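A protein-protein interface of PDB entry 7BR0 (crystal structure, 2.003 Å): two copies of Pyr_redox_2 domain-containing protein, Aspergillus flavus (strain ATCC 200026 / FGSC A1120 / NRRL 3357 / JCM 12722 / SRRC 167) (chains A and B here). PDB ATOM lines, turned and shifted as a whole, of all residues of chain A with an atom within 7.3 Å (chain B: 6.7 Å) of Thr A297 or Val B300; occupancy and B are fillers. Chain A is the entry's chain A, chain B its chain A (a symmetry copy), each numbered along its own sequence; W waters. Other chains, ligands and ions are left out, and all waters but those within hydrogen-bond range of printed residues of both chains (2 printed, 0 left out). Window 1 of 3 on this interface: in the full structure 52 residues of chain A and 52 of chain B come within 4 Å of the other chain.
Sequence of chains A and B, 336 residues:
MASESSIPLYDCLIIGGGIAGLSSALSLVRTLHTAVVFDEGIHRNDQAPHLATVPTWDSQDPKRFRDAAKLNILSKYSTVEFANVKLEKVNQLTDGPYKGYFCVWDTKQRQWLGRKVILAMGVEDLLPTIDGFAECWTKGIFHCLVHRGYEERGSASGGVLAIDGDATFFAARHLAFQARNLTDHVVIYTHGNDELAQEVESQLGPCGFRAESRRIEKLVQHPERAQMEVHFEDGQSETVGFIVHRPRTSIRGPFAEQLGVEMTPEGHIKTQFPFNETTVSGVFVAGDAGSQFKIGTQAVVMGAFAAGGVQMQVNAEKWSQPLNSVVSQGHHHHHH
Thr A53 touches Ser B27 (CG2 to OG, 3.9 Å).
Pro A55 touches Phe B65 (CB to CZ, 3.6 Å).
Pro A55 touches Val B300 (CD to CG1, 3.8 Å).
Phe A293 touches Phe B305.
CD1 of Ile A295 touches CE2 of Phe B305, 3.9 Å away.
Thr A297 touches Val B300 (CG2 to CG1, 3.8 Å).
Val B301 touches Gln A298 (CG2 to OE1, 3.7 Å).
Val A301 touches Thr B297.
OE1 of Gln B298 touches CG2 of Val A301 (3.7 Å).
Val A301 touches Val B301 (CG1 to CG1, 3.95 Å).
Water W2 lies within hydrogen-bond range of the backbone carbonyl oxygen of Thr A53 (2.7 Å), the side-chain hydroxyl of Ser B27 (2.8 Å) and the backbone carbonyl oxygen of Ser B23 (2.9 Å).
Water W1 bridges O of Thr B297 and O of Thr A297.
His A147 touches none of the printed residues of chain B.
Of the printed residues of chain B, Ile A295 touches Phe B305.
Of chain B, only Val B300 (3.8 Å), Val B301 (3.9 Å) and Ala B304 (3.9 Å) come within 4 Å of Thr A297.
Printed residues of chain A within 4 Å of Phe B65: Pro A55 (3.6 Å).
Of the printed residues of chain A, Gln B298 touches Val A301 (3.7 Å).
No residue of chain A comes within 4 Å of Ala B299.
Val B300 touches just these residues of chain A: Pro A55 and Thr A297.
Of the printed residues of chain A, Val B301 touches Thr A297 (3.9 Å), Gln A298 (3.7 Å) and Val A301 (3.95 Å).
Of the printed residues of chain A, Ala B304 touches Thr A297 (3.9 Å).
The nearest residue of chain B that does not touch Thr A297 is Phe B305 (5.0 Å).
The nearest residue of chain A that does not touch Val B300 is Thr A53 (4.7 Å).
The side-chain hydroxyl (OG) of Ser B23 lies within hydrogen-bond range of the backbone carbonyl oxygen (O) of Val B300, 2.7 Å away.
Printed residues of chain A that touch a printed residue of chain B: Thr A53, Pro A55, Phe A293, Ile A295, Thr A297, Gln A298, Val A300 and Val A301.
Hydrophobic or aromatic side chains of chain A that line the printed part of chain B: Pro A55, Phe A293, Ile A295, Val A300 and Val A301.
Among the printed residues, 13 pairs touch across the chains.
Among the printed residues, no Asp or Glu carboxylate lies within 4 Å of a Lys or Arg side-chain nitrogen of the other chain.
Thr A297 touches Val B300, and with the chains exchanged Val A300 touches Thr B297.
Thr A297 touches Val B301, and with the chains exchanged Val A301 touches Thr B297.
Gln A298 touches Val B301, and with the chains exchanged Val A301 touches Gln B298.
Val B301 touches its own counterpart, Val A301.
11 positions are printed for both chains.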
ATOM      1  N   ILE A  19       7.900   4.638  11.702  1.00  0.00           N
ATOM      2  CA  ILE A  19       7.622   5.114  13.047  1.00  0.00           C
ATOM      3  C   ILE A  19       7.998   6.593  13.168  1.00  0.00           C
ATOM      4  O   ILE A  19       7.243   7.384  13.733  1.00  0.00           O
ATOM      5  CB  ILE A  19       8.376   4.282  14.108  1.00  0.00           C
ATOM      6  CG1 ILE A  19       7.941   2.809  14.028  1.00  0.00           C
ATOM      7  CG2 ILE A  19       8.118   4.841  15.510  1.00  0.00           C
ATOM      8  CD1 ILE A  19       8.654   1.870  15.005  1.00  0.00           C
ATOM      9  N   LEU A  51       6.260  -6.094  17.839  1.00  0.00           N
ATOM     10  CA  LEU A  51       6.929  -4.850  18.201  1.00  0.00           C
ATOM     11  C   LEU A  51       7.150  -4.834  19.711  1.00  0.00           C
ATOM     12  O   LEU A  51       6.251  -5.192  20.469  1.00  0.00           O
ATOM     13  CB  LEU A  51       6.091  -3.645  17.757  1.00  0.00           C
ATOM     14  CG  LEU A  51       6.648  -2.241  18.001  1.00  0.00           C
ATOM     15  CD1 LEU A  51       7.943  -2.031  17.239  1.00  0.00           C
ATOM     16  CD2 LEU A  51       5.618  -1.185  17.605  1.00  0.00           C
ATOM     17  N   ALA A  52       8.342  -4.427  20.139  1.00  0.00           N
ATOM     18  CA  ALA A  52       8.694  -4.417  21.559  1.00  0.00           C
ATOM     19  C   ALA A  52       9.176  -3.043  22.016  1.00  0.00           C
ATOM     20  O   ALA A  52       9.633  -2.238  21.208  1.00  0.00           O
ATOM     21  CB  ALA A  52       9.760  -5.465  21.842  1.00  0.00           C
ATOM     22  N   THR A  53       9.062  -2.808  23.324  1.00  0.00           N
ATOM     23  CA  THR A  53       9.519  -1.590  24.017  1.00  0.00           C
ATOM     24  C   THR A  53       8.601  -0.374  23.839  1.00  0.00           C
ATOM     25  O   THR A  53       8.778   0.630  24.528  1.00  0.00           O
ATOM     26  CB  THR A  53      10.954  -1.153  23.591  1.00  0.00           C
ATOM     27  OG1 THR A  53      10.922  -0.459  22.333  1.00  0.00           O
ATOM     28  CG2 THR A  53      11.912  -2.346  23.533  1.00  0.00           C
ATOM     29  N   VAL A  54       7.629  -0.456  22.934  1.00  0.00           N
ATOM     30  CA  VAL A  54       6.667   0.634  22.746  1.00  0.00           C
ATOM     31  C   VAL A  54       5.413   0.364  23.591  1.00  0.00           C
ATOM     32  O   VAL A  54       4.704  -0.607  23.337  1.00  0.00           O
ATOM     33  CB  VAL A  54       6.274   0.799  21.264  1.00  0.00           C
ATOM     34  CG1 VAL A  54       5.264   1.936  21.096  1.00  0.00           C
ATOM     35  CG2 VAL A  54       7.514   1.058  20.408  1.00  0.00           C
ATOM     36  N   PRO A  55       5.135   1.219  24.597  1.00  0.00           N
ATOM     37  CA  PRO A  55       4.020   0.965  25.525  1.00  0.00           C
ATOM     38  C   PRO A  55       2.685   0.637  24.850  1.00  0.00           C
ATOM     39  O   PRO A  55       2.302   1.277  23.867  1.00  0.00           O
ATOM     40  CB  PRO A  55       3.918   2.277  26.312  1.00  0.00           C
ATOM     41  CG  PRO A  55       5.306   2.810  26.308  1.00  0.00           C
ATOM     42  CD  PRO A  55       5.883   2.434  24.970  1.00  0.00           C
ATOM     43  N   HIS A 147      14.394  -6.877  21.798  1.00  0.00           N
ATOM     44  CA  HIS A 147      13.273  -6.926  20.862  1.00  0.00           C
ATOM     45  C   HIS A 147      12.857  -8.360  20.538  1.00  0.00           C
ATOM     46  O   HIS A 147      11.710  -8.612  20.187  1.00  0.00           O
ATOM     47  CB  HIS A 147      13.633  -6.181  19.576  1.00  0.00           C
ATOM     48  CG  HIS A 147      14.015  -4.751  19.799  1.00  0.00           C
ATOM     49  ND1 HIS A 147      14.505  -3.943  18.795  1.00  0.00           N
ATOM     50  CD2 HIS A 147      13.976  -3.982  20.913  1.00  0.00           C
ATOM     51  CE1 HIS A 147      14.751  -2.740  19.280  1.00  0.00           C
ATOM     52  NE2 HIS A 147      14.440  -2.737  20.564  1.00  0.00           N
ATOM     53  N   PHE A 293      21.340   4.999  17.695  1.00  0.00           N
ATOM     54  CA  PHE A 293      20.405   4.114  18.383  1.00  0.00           C
ATOM     55  C   PHE A 293      19.180   3.912  17.514  1.00  0.00           C
ATOM     56  O   PHE A 293      18.204   4.657  17.604  1.00  0.00           O
ATOM     57  CB  PHE A 293      20.020   4.686  19.746  1.00  0.00           C
ATOM     58  CG  PHE A 293      21.202   5.064  20.584  1.00  0.00           C
ATOM     59  CD1 PHE A 293      22.005   4.087  21.144  1.00  0.00           C
ATOM     60  CD2 PHE A 293      21.518   6.394  20.801  1.00  0.00           C
ATOM     61  CE1 PHE A 293      23.101   4.429  21.909  1.00  0.00           C
ATOM     62  CE2 PHE A 293      22.613   6.741  21.564  1.00  0.00           C
ATOM     63  CZ  PHE A 293      23.403   5.758  22.119  1.00  0.00           C
ATOM     64  N   LYS A 294      19.248   2.894  16.668  1.00  0.00           N
ATOM     65  CA  LYS A 294      18.260   2.693  15.625  1.00  0.00           C
ATOM     66  C   LYS A 294      17.121   1.823  16.137  1.00  0.00           C
ATOM     67  O   LYS A 294      16.925   0.695  15.678  1.00  0.00           O
ATOM     68  CB  LYS A 294      18.936   2.082  14.398  1.00  0.00           C
ATOM     69  CG  LYS A 294      20.037   2.979  13.850  1.00  0.00           C
ATOM     70  CD  LYS A 294      20.817   2.332  12.729  1.00  0.00           C
ATOM     71  CE  LYS A 294      21.745   3.341  12.093  1.00  0.00           C
ATOM     72  NZ  LYS A 294      22.757   3.860  13.041  1.00  0.00           N
ATOM     73  N   ILE A 295      16.377   2.377  17.091  1.00  0.00           N
ATOM     74  CA  ILE A 295      15.287   1.675  17.763  1.00  0.00           C
ATOM     75  C   ILE A 295      13.988   2.471  17.696  1.00  0.00           C
ATOM     76  O   ILE A 295      13.992   3.668  17.401  1.00  0.00           O
ATOM     77  CB  ILE A 295      15.639   1.396  19.236  1.00  0.00           C
ATOM     78  CG1 ILE A 295      15.833   2.706  20.005  1.00  0.00           C
ATOM     79  CG2 ILE A 295      16.893   0.528  19.307  1.00  0.00           C
ATOM     80  CD1 ILE A 295      16.118   2.521  21.477  1.00  0.00           C
ATOM     81  N   GLY A 296      12.878   1.805  17.998  1.00  0.00           N
ATOM     82  CA  GLY A 296      11.561   2.384  17.802  1.00  0.00           C
ATOM     83  C   GLY A 296      11.237   3.586  18.673  1.00  0.00           C
ATOM     84  O   GLY A 296      10.674   4.564  18.187  1.00  0.00           O
ATOM     85  N   THR A 297      11.579   3.520  19.957  1.00  0.00           N
ATOM     86  CA  THR A 297      11.267   4.615  20.873  1.00  0.00           C
ATOM     87  C   THR A 297      12.060   5.864  20.500  1.00  0.00           C
ATOM     88  O   THR A 297      11.584   6.990  20.669  1.00  0.00           O
ATOM     89  CB  THR A 297      11.559   4.233  22.339  1.00  0.00           C
ATOM     90  OG1 THR A 297      12.921   3.807  22.471  1.00  0.00           O
ATOM     91  CG2 THR A 297      10.630   3.114  22.794  1.00  0.00           C
ATOM     92  N   GLN A 298      13.268   5.662  19.984  1.00  0.00           N
ATOM     93  CA  GLN A 298      14.088   6.766  19.494  1.00  0.00           C
ATOM     94  C   GLN A 298      13.437   7.397  18.262  1.00  0.00           C
ATOM     95  O   GLN A 298      13.428   8.618  18.107  1.00  0.00           O
ATOM     96  CB  GLN A 298      15.503   6.278  19.164  1.00  0.00           C
ATOM     97  CG  GLN A 298      16.445   7.341  18.600  1.00  0.00           C
ATOM     98  CD  GLN A 298      16.951   8.311  19.645  1.00  0.00           C
ATOM     99  OE1 GLN A 298      16.269   8.608  20.622  1.00  0.00           O
ATOM    100  NE2 GLN A 298      18.164   8.806  19.444  1.00  0.00           N
ATOM    101  N   ALA A 299      12.891   6.558  17.391  1.00  0.00           N
ATOM    102  CA  ALA A 299      12.204   7.045  16.199  1.00  0.00           C
ATOM    103  C   ALA A 299      11.021   7.938  16.579  1.00  0.00           C
ATOM    104  O   ALA A 299      10.812   8.995  15.980  1.00  0.00           O
ATOM    105  CB  ALA A 299      11.733   5.880  15.341  1.00  0.00           C
ATOM    106  N   VAL A 300      10.251   7.505  17.574  1.00  0.00           N
ATOM    107  CA  VAL A 300       9.089   8.266  18.034  1.00  0.00           C
ATOM    108  C   VAL A 300       9.487   9.642  18.562  1.00  0.00           C
ATOM    109  O   VAL A 300       8.929  10.656  18.144  1.00  0.00           O
ATOM    110  CB  VAL A 300       8.316   7.504  19.138  1.00  0.00           C
ATOM    111  CG1 VAL A 300       7.170   8.348  19.690  1.00  0.00           C
ATOM    112  CG2 VAL A 300       7.772   6.198  18.592  1.00  0.00           C
ATOM    113  N   VAL A 301      10.445   9.684  19.482  1.00  0.00           N
ATOM    114  CA  VAL A 301      10.823  10.954  20.093  1.00  0.00           C
ATOM    115  C   VAL A 301      11.487  11.880  19.068  1.00  0.00           C
ATOM    116  O   VAL A 301      11.254  13.089  19.085  1.00  0.00           O
ATOM    117  CB  VAL A 301      11.763  10.750  21.318  1.00  0.00           C
ATOM    118  CG1 VAL A 301      13.116  10.199  20.901  1.00  0.00           C
ATOM    119  CG2 VAL A 301      11.935  12.057  22.086  1.00  0.00           C
ATOM    120  N   MET A 302      12.291  11.323  18.164  1.00  0.00           N
ATOM    121  CA  MET A 302      12.953  12.144  17.151  1.00  0.00           C
ATOM    122  C   MET A 302      11.933  12.768  16.203  1.00  0.00           C
ATOM    123  O   MET A 302      12.116  13.892  15.742  1.00  0.00           O
ATOM    124  CB  MET A 302      13.966  11.328  16.347  1.00  0.00           C
ATOM    125  CG  MET A 302      15.270  11.035  17.078  1.00  0.00           C
ATOM    126  SD  MET A 302      16.493  10.286  15.984  1.00  0.00           S
ATOM    127  CE  MET A 302      17.153  11.744  15.177  1.00  0.00           C
ATOM    128  N   GLY A 303      10.862  12.037  15.912  1.00  0.00           N
ATOM    129  CA  GLY A 303       9.814  12.550  15.047  1.00  0.00           C
ATOM    130  C   GLY A 303       9.104  13.733  15.675  1.00  0.00           C
ATOM    131  O   GLY A 303       8.773  14.712  14.999  1.00  0.00           O
ATOM    132  N   ILE B  19       4.645   7.364  32.762  1.00  0.00           N
ATOM    133  CA  ILE B  19       5.066   6.965  31.429  1.00  0.00           C
ATOM    134  C   ILE B  19       6.513   6.468  31.462  1.00  0.00           C
ATOM    135  O   ILE B  19       6.835   5.444  30.861  1.00  0.00           O
ATOM    136  CB  ILE B  19       4.922   8.126  30.420  1.00  0.00           C
ATOM    137  CG1 ILE B  19       3.453   8.572  30.339  1.00  0.00           C
ATOM    138  CG2 ILE B  19       5.430   7.701  29.040  1.00  0.00           C
ATOM    139  CD1 ILE B  19       3.188   9.754  29.399  1.00  0.00           C
ATOM    140  N   ALA B  20       7.373   7.179  32.186  1.00  0.00           N
ATOM    141  CA  ALA B  20       8.785   6.819  32.264  1.00  0.00           C
ATOM    142  C   ALA B  20       8.985   5.474  32.957  1.00  0.00           C
ATOM    143  O   ALA B  20       9.697   4.608  32.451  1.00  0.00           O
ATOM    144  CB  ALA B  20       9.564   7.897  32.984  1.00  0.00           C
ATOM    145  N   SER B  23       7.680   2.521  30.951  1.00  0.00           N
ATOM    146  CA  SER B  23       8.504   2.235  29.790  1.00  0.00           C
ATOM    147  C   SER B  23       9.757   1.464  30.207  1.00  0.00           C
ATOM    148  O   SER B  23      10.174   0.539  29.515  1.00  0.00           O
ATOM    149  CB  SER B  23       8.875   3.530  29.062  1.00  0.00           C
ATOM    150  OG  SER B  23       9.684   3.247  27.938  1.00  0.00           O
ATOM    151  N   SER B  24      10.340   1.834  31.346  1.00  0.00           N
ATOM    152  CA  SER B  24      11.487   1.105  31.889  1.00  0.00           C
ATOM    153  C   SER B  24      11.124  -0.349  32.180  1.00  0.00           C
ATOM    154  O   SER B  24      11.853  -1.272  31.807  1.00  0.00           O
ATOM    155  CB  SER B  24      12.003   1.774  33.166  1.00  0.00           C
ATOM    156  OG  SER B  24      12.576   3.038  32.888  1.00  0.00           O
ATOM    157  N   SER B  27      10.817  -2.614  29.083  1.00  0.00           N
ATOM    158  CA  SER B  27      12.088  -3.081  28.527  1.00  0.00           C
ATOM    159  C   SER B  27      12.711  -4.167  29.408  1.00  0.00           C
ATOM    160  O   SER B  27      13.296  -5.125  28.900  1.00  0.00           O
ATOM    161  CB  SER B  27      13.069  -1.917  28.357  1.00  0.00           C
ATOM    162  OG  SER B  27      12.780  -1.166  27.185  1.00  0.00           O
ATOM    163  N   VAL B  54       1.738  10.747  21.261  1.00  0.00           N
ATOM    164  CA  VAL B  54       2.097   9.331  21.398  1.00  0.00           C
ATOM    165  C   VAL B  54       1.304   8.500  20.379  1.00  0.00           C
ATOM    166  O   VAL B  54       0.081   8.429  20.469  1.00  0.00           O
ATOM    167  CB  VAL B  54       1.827   8.810  22.823  1.00  0.00           C
ATOM    168  CG1 VAL B  54       2.202   7.331  22.937  1.00  0.00           C
ATOM    169  CG2 VAL B  54       2.603   9.635  23.850  1.00  0.00           C
ATOM    170  N   PHE B  65      -4.197   4.944  28.880  1.00  0.00           N
ATOM    171  CA  PHE B  65      -2.885   4.641  28.316  1.00  0.00           C
ATOM    172  C   PHE B  65      -2.013   3.917  29.341  1.00  0.00           C
ATOM    173  O   PHE B  65      -1.435   2.871  29.040  1.00  0.00           O
ATOM    174  CB  PHE B  65      -2.183   5.917  27.835  1.00  0.00           C
ATOM    175  CG  PHE B  65      -0.749   5.700  27.432  1.00  0.00           C
ATOM    176  CD1 PHE B  65      -0.438   5.037  26.255  1.00  0.00           C
ATOM    177  CD2 PHE B  65       0.284   6.151  28.235  1.00  0.00           C
ATOM    178  CE1 PHE B  65       0.880   4.832  25.887  1.00  0.00           C
ATOM    179  CE2 PHE B  65       1.603   5.948  27.872  1.00  0.00           C
ATOM    180  CZ  PHE B  65       1.902   5.288  26.697  1.00  0.00           C
ATOM    181  N   GLY B 287      12.267  10.437  32.456  1.00  0.00           N
ATOM    182  CA  GLY B 287      11.062  11.240  32.484  1.00  0.00           C
ATOM    183  C   GLY B 287      11.320  12.685  32.863  1.00  0.00           C
ATOM    184  O   GLY B 287      12.446  13.180  32.745  1.00  0.00           O
ATOM    185  N   ILE B 295       8.065  16.032  28.382  1.00  0.00           N
ATOM    186  CA  ILE B 295       6.980  15.563  27.526  1.00  0.00           C
ATOM    187  C   ILE B 295       6.928  14.039  27.478  1.00  0.00           C
ATOM    188  O   ILE B 295       7.885  13.360  27.855  1.00  0.00           O
ATOM    189  CB  ILE B 295       7.131  16.113  26.096  1.00  0.00           C
ATOM    190  CG1 ILE B 295       8.425  15.604  25.453  1.00  0.00           C
ATOM    191  CG2 ILE B 295       7.100  17.639  26.129  1.00  0.00           C
ATOM    192  CD1 ILE B 295       8.618  16.046  24.021  1.00  0.00           C
ATOM    193  N   GLY B 296       5.813  13.507  26.988  1.00  0.00           N
ATOM    194  CA  GLY B 296       5.555  12.079  27.050  1.00  0.00           C
ATOM    195  C   GLY B 296       6.492  11.207  26.231  1.00  0.00           C
ATOM    196  O   GLY B 296       6.935  10.164  26.707  1.00  0.00           O
ATOM    197  N   THR B 297       6.790  11.618  25.001  1.00  0.00           N
ATOM    198  CA  THR B 297       7.650  10.819  24.132  1.00  0.00           C
ATOM    199  C   THR B 297       9.068  10.760  24.693  1.00  0.00           C
ATOM    200  O   THR B 297       9.767   9.754  24.543  1.00  0.00           O
ATOM    201  CB  THR B 297       7.683  11.375  22.693  1.00  0.00           C
ATOM    202  OG1 THR B 297       8.084  12.751  22.711  1.00  0.00           O
ATOM    203  CG2 THR B 297       6.309  11.255  22.043  1.00  0.00           C
ATOM    204  N   GLN B 298       9.487  11.839  25.346  1.00  0.00           N
ATOM    205  CA  GLN B 298      10.783  11.874  26.016  1.00  0.00           C
ATOM    206  C   GLN B 298      10.794  10.898  27.193  1.00  0.00           C
ATOM    207  O   GLN B 298      11.783  10.205  27.432  1.00  0.00           O
ATOM    208  CB  GLN B 298      11.101  13.296  26.493  1.00  0.00           C
ATOM    209  CG  GLN B 298      12.421  13.450  27.249  1.00  0.00           C
ATOM    210  CD  GLN B 298      13.637  13.408  26.350  1.00  0.00           C
ATOM    211  OE1 GLN B 298      13.642  12.746  25.315  1.00  0.00           O
ATOM    212  NE2 GLN B 298      14.680  14.127  26.743  1.00  0.00           N
ATOM    213  N   ALA B 299       9.688  10.847  27.925  1.00  0.00           N
ATOM    214  CA  ALA B 299       9.564   9.923  29.047  1.00  0.00           C
ATOM    215  C   ALA B 299       9.714   8.475  28.580  1.00  0.00           C
ATOM    216  O   ALA B 299      10.401   7.674  29.220  1.00  0.00           O
ATOM    217  CB  ALA B 299       8.229  10.117  29.752  1.00  0.00           C
ATOM    218  N   VAL B 300       9.067   8.144  27.465  1.00  0.00           N
ATOM    219  CA  VAL B 300       9.130   6.792  26.912  1.00  0.00           C
ATOM    220  C   VAL B 300      10.557   6.398  26.539  1.00  0.00           C
ATOM    221  O   VAL B 300      11.042   5.346  26.951  1.00  0.00           O
ATOM    222  CB  VAL B 300       8.223   6.649  25.665  1.00  0.00           C
ATOM    223  CG1 VAL B 300       8.375   5.269  25.029  1.00  0.00           C
ATOM    224  CG2 VAL B 300       6.772   6.880  26.042  1.00  0.00           C
ATOM    225  N   VAL B 301      11.231   7.236  25.757  1.00  0.00           N
ATOM    226  CA  VAL B 301      12.570   6.890  25.291  1.00  0.00           C
ATOM    227  C   VAL B 301      13.565   6.857  26.457  1.00  0.00           C
ATOM    228  O   VAL B 301      14.445   5.997  26.495  1.00  0.00           O
ATOM    229  CB  VAL B 301      13.070   7.870  24.188  1.00  0.00           C
ATOM    230  CG1 VAL B 301      13.291   9.268  24.739  1.00  0.00           C
ATOM    231  CG2 VAL B 301      14.349   7.344  23.543  1.00  0.00           C
ATOM    232  N   MET B 302      13.419   7.769  27.417  1.00  0.00           N
ATOM    233  CA  MET B 302      14.328   7.794  28.564  1.00  0.00           C
ATOM    234  C   MET B 302      14.169   6.535  29.412  1.00  0.00           C
ATOM    235  O   MET B 302      15.142   6.033  29.970  1.00  0.00           O
ATOM    236  CB  MET B 302      14.094   9.029  29.433  1.00  0.00           C
ATOM    237  CG  MET B 302      14.653  10.325  28.861  1.00  0.00           C
ATOM    238  SD  MET B 302      14.550  11.678  30.049  1.00  0.00           S
ATOM    239  CE  MET B 302      16.013  11.362  31.036  1.00  0.00           C
ATOM    240  N   GLY B 303      12.944   6.029  29.508  1.00  0.00           N
ATOM    241  CA  GLY B 303      12.689   4.814  30.263  1.00  0.00           C
ATOM    242  C   GLY B 303      13.369   3.615  29.632  1.00  0.00           C
ATOM    243  O   GLY B 303      13.914   2.752  30.326  1.00  0.00           O
ATOM    244  N   ALA B 304      13.346   3.567  28.304  1.00  0.00           N
ATOM    245  CA  ALA B 304      13.974   2.480  27.567  1.00  0.00           C
ATOM    246  C   ALA B 304      15.491   2.504  27.753  1.00  0.00           C
ATOM    247  O   ALA B 304      16.110   1.462  27.947  1.00  0.00           O
ATOM    248  CB  ALA B 304      13.616   2.563  26.084  1.00  0.00           C
ATOM    249  N   PHE B 305      16.089   3.691  27.707  1.00  0.00           N
ATOM    250  CA  PHE B 305      17.538   3.799  27.832  1.00  0.00           C
ATOM    251  C   PHE B 305      17.997   3.585  29.282  1.00  0.00           C
ATOM    252  O   PHE B 305      19.050   3.000  29.515  1.00  0.00           O
ATOM    253  CB  PHE B 305      18.021   5.149  27.301  1.00  0.00           C
ATOM    254  CG  PHE B 305      18.248   5.165  25.809  1.00  0.00           C
ATOM    255  CD1 PHE B 305      19.461   4.752  25.275  1.00  0.00           C
ATOM    256  CD2 PHE B 305      17.248   5.573  24.942  1.00  0.00           C
ATOM    257  CE1 PHE B 305      19.674   4.756  23.908  1.00  0.00           C
ATOM    258  CE2 PHE B 305      17.454   5.581  23.572  1.00  0.00           C
ATOM    259  CZ  PHE B 305      18.669   5.170  23.055  1.00  0.00           C
HETATM  260  O   HOH W   1       9.330   7.648  22.491  1.00  0.00           O
HETATM  261  O   HOH W   2      10.480   0.346  26.656  1.00  0.00           O
